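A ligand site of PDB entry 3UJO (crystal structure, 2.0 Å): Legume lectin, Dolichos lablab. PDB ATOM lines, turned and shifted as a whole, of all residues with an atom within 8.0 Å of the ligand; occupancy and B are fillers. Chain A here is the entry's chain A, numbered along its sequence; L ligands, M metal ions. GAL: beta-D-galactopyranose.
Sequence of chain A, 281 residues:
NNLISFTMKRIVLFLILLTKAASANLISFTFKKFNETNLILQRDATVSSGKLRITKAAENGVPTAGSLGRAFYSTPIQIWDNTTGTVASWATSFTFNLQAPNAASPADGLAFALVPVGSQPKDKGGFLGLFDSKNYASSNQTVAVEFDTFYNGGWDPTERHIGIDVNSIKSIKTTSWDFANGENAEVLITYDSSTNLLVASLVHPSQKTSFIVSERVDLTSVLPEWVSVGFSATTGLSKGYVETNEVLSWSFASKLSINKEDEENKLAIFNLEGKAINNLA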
ATOM      1  N   SER A 105      18.083  34.353  11.554  1.00  0.00           N
ATOM      2  CA  SER A 105      18.936  33.719  12.564  1.00  0.00           C
ATOM      3  C   SER A 105      18.644  34.210  13.996  1.00  0.00           C
ATOM      4  O   SER A 105      19.394  35.030  14.542  1.00  0.00           O
ATOM      5  CB  SER A 105      20.417  33.917  12.214  1.00  0.00           C
ATOM      6  OG  SER A 105      20.768  35.287  12.210  1.00  0.00           O
ATOM      7  N   PRO A 106      17.544  33.718  14.608  1.00  0.00           N
ATOM      8  CA  PRO A 106      17.212  34.087  15.991  1.00  0.00           C
ATOM      9  C   PRO A 106      17.485  32.979  17.019  1.00  0.00           C
ATOM     10  O   PRO A 106      17.056  31.835  16.840  1.00  0.00           O
ATOM     11  CB  PRO A 106      15.713  34.378  15.899  1.00  0.00           C
ATOM     12  CG  PRO A 106      15.220  33.578  14.689  1.00  0.00           C
ATOM     13  CD  PRO A 106      16.422  33.022  13.963  1.00  0.00           C
ATOM     14  N   ALA A 107      18.195  33.343  18.099  1.00  0.00           N
ATOM     15  CA  ALA A 107      18.481  32.419  19.205  1.00  0.00           C
ATOM     16  C   ALA A 107      18.840  33.192  20.485  1.00  0.00           C
ATOM     17  O   ALA A 107      19.667  34.107  20.429  1.00  0.00           O
ATOM     18  CB  ALA A 107      19.609  31.464  18.843  1.00  0.00           C
ATOM     19  N   ASP A 108      18.230  32.855  21.617  1.00  0.00           N
ATOM     20  CA  ASP A 108      17.229  31.787  21.733  1.00  0.00           C
ATOM     21  C   ASP A 108      15.884  32.336  22.210  1.00  0.00           C
ATOM     22  O   ASP A 108      14.833  31.970  21.679  1.00  0.00           O
ATOM     23  CB  ASP A 108      17.704  30.695  22.706  1.00  0.00           C
ATOM     24  CG  ASP A 108      18.813  29.837  22.130  1.00  0.00           C
ATOM     25  OD1 ASP A 108      18.590  29.172  21.106  1.00  0.00           O
ATOM     26  OD2 ASP A 108      19.911  29.826  22.732  1.00  0.00           O
ATOM     27  N   LYS A 124      23.633  27.135  29.394  1.00  0.00           N
ATOM     28  CA  LYS A 124      23.146  28.168  28.479  1.00  0.00           C
ATOM     29  C   LYS A 124      22.842  27.594  27.096  1.00  0.00           C
ATOM     30  O   LYS A 124      23.223  26.460  26.787  1.00  0.00           O
ATOM     31  CB  LYS A 124      24.189  29.287  28.349  1.00  0.00           C
ATOM     32  CG  LYS A 124      24.611  29.919  29.665  1.00  0.00           C
ATOM     33  CD  LYS A 124      25.837  30.812  29.483  1.00  0.00           C
ATOM     34  CE  LYS A 124      26.324  31.366  30.819  1.00  0.00           C
ATOM     35  NZ  LYS A 124      26.906  30.314  31.710  1.00  0.00           N
ATOM     36  N   GLY A 125      22.147  28.378  26.283  1.00  0.00           N
ATOM     37  CA  GLY A 125      21.842  28.000  24.910  1.00  0.00           C
ATOM     38  C   GLY A 125      20.492  27.324  24.743  1.00  0.00           C
ATOM     39  O   GLY A 125      19.443  27.934  24.960  1.00  0.00           O
ATOM     40  N   GLY A 126      20.533  26.046  24.362  1.00  0.00           N
ATOM     41  CA  GLY A 126      19.319  25.241  24.185  1.00  0.00           C
ATOM     42  C   GLY A 126      18.587  24.948  25.476  1.00  0.00           C
ATOM     43  O   GLY A 126      17.360  24.810  25.479  1.00  0.00           O
ATOM     44  N   PHE A 127      19.335  24.856  26.567  1.00  0.00           N
ATOM     45  CA  PHE A 127      18.766  24.594  27.893  1.00  0.00           C
ATOM     46  C   PHE A 127      18.135  25.844  28.525  1.00  0.00           C
ATOM     47  O   PHE A 127      17.491  25.754  29.573  1.00  0.00           O
ATOM     48  CB  PHE A 127      19.832  24.005  28.821  1.00  0.00           C
ATOM     49  CG  PHE A 127      20.370  22.681  28.364  1.00  0.00           C
ATOM     50  CD1 PHE A 127      19.681  21.498  28.625  1.00  0.00           C
ATOM     51  CD2 PHE A 127      21.583  22.603  27.666  1.00  0.00           C
ATOM     52  CE1 PHE A 127      20.178  20.273  28.196  1.00  0.00           C
ATOM     53  CE2 PHE A 127      22.089  21.377  27.240  1.00  0.00           C
ATOM     54  CZ  PHE A 127      21.382  20.211  27.500  1.00  0.00           C
ATOM     55  N   LEU A 128      18.335  26.993  27.872  1.00  0.00           N
ATOM     56  CA  LEU A 128      17.734  28.283  28.259  1.00  0.00           C
ATOM     57  C   LEU A 128      18.089  28.764  29.670  1.00  0.00           C
ATOM     58  O   LEU A 128      17.365  29.573  30.253  1.00  0.00           O
ATOM     59  CB  LEU A 128      16.209  28.255  28.052  1.00  0.00           C
ATOM     60  CG  LEU A 128      15.648  28.210  26.632  1.00  0.00           C
ATOM     61  CD1 LEU A 128      14.212  27.695  26.639  1.00  0.00           C
ATOM     62  CD2 LEU A 128      15.734  29.559  25.937  1.00  0.00           C
ATOM     63  N   PHE A 150      14.757  29.489  18.107  1.00  0.00           N
ATOM     64  CA  PHE A 150      15.722  28.644  17.398  1.00  0.00           C
ATOM     65  C   PHE A 150      15.254  27.192  17.261  1.00  0.00           C
ATOM     66  O   PHE A 150      14.557  26.674  18.139  1.00  0.00           O
ATOM     67  CB  PHE A 150      17.097  28.710  18.070  1.00  0.00           C
ATOM     68  CG  PHE A 150      18.225  28.242  17.187  1.00  0.00           C
ATOM     69  CD1 PHE A 150      18.769  26.972  17.347  1.00  0.00           C
ATOM     70  CD2 PHE A 150      18.729  29.069  16.191  1.00  0.00           C
ATOM     71  CE1 PHE A 150      19.816  26.539  16.527  1.00  0.00           C
ATOM     72  CE2 PHE A 150      19.778  28.644  15.366  1.00  0.00           C
ATOM     73  CZ  PHE A 150      20.309  27.373  15.537  1.00  0.00           C
ATOM     74  N   TYR A 151      15.646  26.564  16.161  1.00  0.00           N
ATOM     75  CA  TYR A 151      15.293  25.174  15.882  1.00  0.00           C
ATOM     76  C   TYR A 151      16.406  24.211  16.325  1.00  0.00           C
ATOM     77  O   TYR A 151      17.488  24.189  15.742  1.00  0.00           O
ATOM     78  CB  TYR A 151      14.988  24.999  14.385  1.00  0.00           C
ATOM     79  CG  TYR A 151      14.757  23.566  13.947  1.00  0.00           C
ATOM     80  CD1 TYR A 151      13.559  22.909  14.223  1.00  0.00           C
ATOM     81  CD2 TYR A 151      15.738  22.877  13.228  1.00  0.00           C
ATOM     82  CE1 TYR A 151      13.348  21.589  13.825  1.00  0.00           C
ATOM     83  CE2 TYR A 151      15.531  21.560  12.817  1.00  0.00           C
ATOM     84  CZ  TYR A 151      14.342  20.926  13.116  1.00  0.00           C
ATOM     85  OH  TYR A 151      14.135  19.627  12.717  1.00  0.00           O
ATOM     86  N   ASN A 152      16.118  23.444  17.371  1.00  0.00           N
ATOM     87  CA  ASN A 152      17.024  22.404  17.846  1.00  0.00           C
ATOM     88  C   ASN A 152      16.466  21.021  17.515  1.00  0.00           C
ATOM     89  O   ASN A 152      17.091  20.245  16.793  1.00  0.00           O
ATOM     90  CB  ASN A 152      17.291  22.532  19.344  1.00  0.00           C
ATOM     91  CG  ASN A 152      17.916  23.869  19.713  1.00  0.00           C
ATOM     92  OD1 ASN A 152      17.350  24.933  19.453  1.00  0.00           O
ATOM     93  ND2 ASN A 152      19.084  23.820  20.347  1.00  0.00           N
ATOM     94  N   TRP A 155      14.932  18.223  21.660  1.00  0.00           N
ATOM     95  CA  TRP A 155      13.988  18.353  22.772  1.00  0.00           C
ATOM     96  C   TRP A 155      12.842  19.289  22.366  1.00  0.00           C
ATOM     97  O   TRP A 155      11.987  19.633  23.192  1.00  0.00           O
ATOM     98  CB  TRP A 155      14.709  18.884  24.022  1.00  0.00           C
ATOM     99  CG  TRP A 155      15.577  20.085  23.761  1.00  0.00           C
ATOM    100  CD1 TRP A 155      15.201  21.398  23.761  1.00  0.00           C
ATOM    101  CD2 TRP A 155      16.985  20.075  23.446  1.00  0.00           C
ATOM    102  NE1 TRP A 155      16.280  22.202  23.474  1.00  0.00           N
ATOM    103  CE2 TRP A 155      17.379  21.420  23.275  1.00  0.00           C
ATOM    104  CE3 TRP A 155      17.939  19.063  23.310  1.00  0.00           C
ATOM    105  CZ2 TRP A 155      18.699  21.776  22.973  1.00  0.00           C
ATOM    106  CZ3 TRP A 155      19.250  19.416  22.998  1.00  0.00           C
ATOM    107  CH2 TRP A 155      19.612  20.762  22.833  1.00  0.00           C
ATOM    108  N   ASP A 156      12.828  19.664  21.086  1.00  0.00           N
ATOM    109  CA  ASP A 156      11.883  20.649  20.557  1.00  0.00           C
ATOM    110  C   ASP A 156      11.014  20.078  19.431  1.00  0.00           C
ATOM    111  O   ASP A 156      11.380  19.072  18.818  1.00  0.00           O
ATOM    112  CB  ASP A 156      12.656  21.882  20.052  1.00  0.00           C
ATOM    113  CG  ASP A 156      13.292  22.675  21.178  1.00  0.00           C
ATOM    114  OD1 ASP A 156      12.598  23.013  22.159  1.00  0.00           O
ATOM    115  OD2 ASP A 156      14.505  22.974  21.075  1.00  0.00           O
ATOM    116  N   THR A 235      21.067  33.372  25.457  1.00  0.00           N
ATOM    117  CA  THR A 235      21.504  33.503  24.065  1.00  0.00           C
ATOM    118  C   THR A 235      22.204  32.214  23.607  1.00  0.00           C
ATOM    119  O   THR A 235      22.311  31.254  24.371  1.00  0.00           O
ATOM    120  CB  THR A 235      22.444  34.718  23.863  1.00  0.00           C
ATOM    121  OG1 THR A 235      23.476  34.698  24.851  1.00  0.00           O
ATOM    122  CG2 THR A 235      21.662  36.025  23.958  1.00  0.00           C
ATOM    123  N   GLY A 236      22.679  32.206  22.363  1.00  0.00           N
ATOM    124  CA  GLY A 236      23.360  31.042  21.803  1.00  0.00           C
ATOM    125  C   GLY A 236      24.872  31.050  22.008  1.00  0.00           C
ATOM    126  O   GLY A 236      25.403  31.877  22.747  1.00  0.00           O
ATOM    127  N   LEU A 237      25.554  30.121  21.340  1.00  0.00           N
ATOM    128  CA  LEU A 237      27.015  30.003  21.404  1.00  0.00           C
ATOM    129  C   LEU A 237      27.703  30.678  20.217  1.00  0.00           C
ATOM    130  O   LEU A 237      28.917  30.569  20.045  1.00  0.00           O
ATOM    131  CB  LEU A 237      27.441  28.527  21.475  1.00  0.00           C
ATOM    132  CG  LEU A 237      27.352  27.767  22.799  1.00  0.00           C
ATOM    133  CD1 LEU A 237      27.389  26.269  22.552  1.00  0.00           C
ATOM    134  CD2 LEU A 237      28.461  28.181  23.756  1.00  0.00           C
ATOM    135  N   SER A 238      26.912  31.379  19.397  1.00  0.00           N
ATOM    136  CA  SER A 238      27.435  32.014  18.179  1.00  0.00           C
ATOM    137  C   SER A 238      26.908  33.439  18.009  1.00  0.00           C
ATOM    138  O   SER A 238      25.768  33.736  18.359  1.00  0.00           O
ATOM    139  CB  SER A 238      27.096  31.181  16.949  1.00  0.00           C
ATOM    140  OG  SER A 238      27.486  29.825  17.129  1.00  0.00           O
ATOM    141  N   LYS A 239      27.757  34.310  17.452  1.00  0.00           N
ATOM    142  CA  LYS A 239      27.413  35.720  17.245  1.00  0.00           C
ATOM    143  C   LYS A 239      26.420  35.948  16.099  1.00  0.00           C
ATOM    144  O   LYS A 239      25.787  37.002  16.037  1.00  0.00           O
ATOM    145  CB  LYS A 239      28.691  36.541  17.007  1.00  0.00           C
ATOM    146  N   GLY A 240      26.300  34.962  15.213  1.00  0.00           N
ATOM    147  CA  GLY A 240      25.385  35.040  14.074  1.00  0.00           C
ATOM    148  C   GLY A 240      23.921  34.909  14.445  1.00  0.00           C
ATOM    149  O   GLY A 240      23.041  35.418  13.743  1.00  0.00           O
ATOM    150  N   TYR A 241      23.652  34.224  15.560  1.00  0.00           N
ATOM    151  CA  TYR A 241      22.292  33.994  16.040  1.00  0.00           C
ATOM    152  C   TYR A 241      22.028  34.777  17.331  1.00  0.00           C
ATOM    153  O   TYR A 241      22.086  34.225  18.429  1.00  0.00           O
ATOM    154  CB  TYR A 241      22.047  32.494  16.265  1.00  0.00           C
ATOM    155  CG  TYR A 241      22.620  31.577  15.211  1.00  0.00           C
ATOM    156  CD1 TYR A 241      21.907  31.273  14.048  1.00  0.00           C
ATOM    157  CD2 TYR A 241      23.879  30.991  15.371  1.00  0.00           C
ATOM    158  CE1 TYR A 241      22.435  30.437  13.069  1.00  0.00           C
ATOM    159  CE2 TYR A 241      24.414  30.145  14.399  1.00  0.00           C
ATOM    160  CZ  TYR A 241      23.690  29.866  13.254  1.00  0.00           C
ATOM    161  OH  TYR A 241      24.214  29.032  12.297  1.00  0.00           O
HETATM  162  C1  GAL L   1      24.436  24.955  19.667  1.00  0.00           C
HETATM  163  C2  GAL L   1      23.428  25.066  20.818  1.00  0.00           C
HETATM  164  C3  GAL L   1      22.101  25.674  20.330  1.00  0.00           C
HETATM  165  C4  GAL L   1      22.306  26.914  19.445  1.00  0.00           C
HETATM  166  C5  GAL L   1      23.443  26.701  18.431  1.00  0.00           C
HETATM  167  C6  GAL L   1      23.753  27.974  17.657  1.00  0.00           C
HETATM  168  O1  GAL L   1      25.669  24.467  20.153  1.00  0.00           O
HETATM  169  O2  GAL L   1      23.187  23.792  21.377  1.00  0.00           O
HETATM  170  O3  GAL L   1      21.295  25.998  21.435  1.00  0.00           O
HETATM  171  O4  GAL L   1      22.569  28.044  20.260  1.00  0.00           O
HETATM  172  O5  GAL L   1      24.613  26.224  19.067  1.00  0.00           O
HETATM  173  O6  GAL L   1      23.363  27.817  16.315  1.00  0.00           O
HETATM  174 CA    CA M   1      15.209  25.904  21.894  1.00  0.00          CA
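C of Gly 125 touches O3 of the ligand, at 3.7 Å. Phe 150 touches the ligand (CZ to O6, 3.2 Å). Gly 236 touches the ligand (CA to O4, 3.5 Å). Leu 237 touches the ligand. Tyr 241 touches the ligand (CE2 to O6, 3.2 Å). Hydrophobic or aromatic side chains within 4 Å of the ligand: Phe 150, Leu 237 and Tyr 241. Seven residues have an atom within 4 Å of the ligand: Gly 125, Gly 126, Phe 150, Asn 152, Gly 236, Leu 237 and Tyr 241.
ND2 of Asn 152 sits at hydrogen-bond distance from O3 of the ligand (3.3 Å). O3 of the ligand sits at hydrogen-bond distance from N of Gly 126, 3.0 Å away.
The backbone carbonyl oxygen (O) of Gly 126 lies within hydrogen-bond range of the indole nitrogen (NE1) of Trp 155 (3.5 Å). The backbone NH (N) of Gly 125 lies close to the backbone carbonyl oxygen (O) of Thr 235 (3.5 Å).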
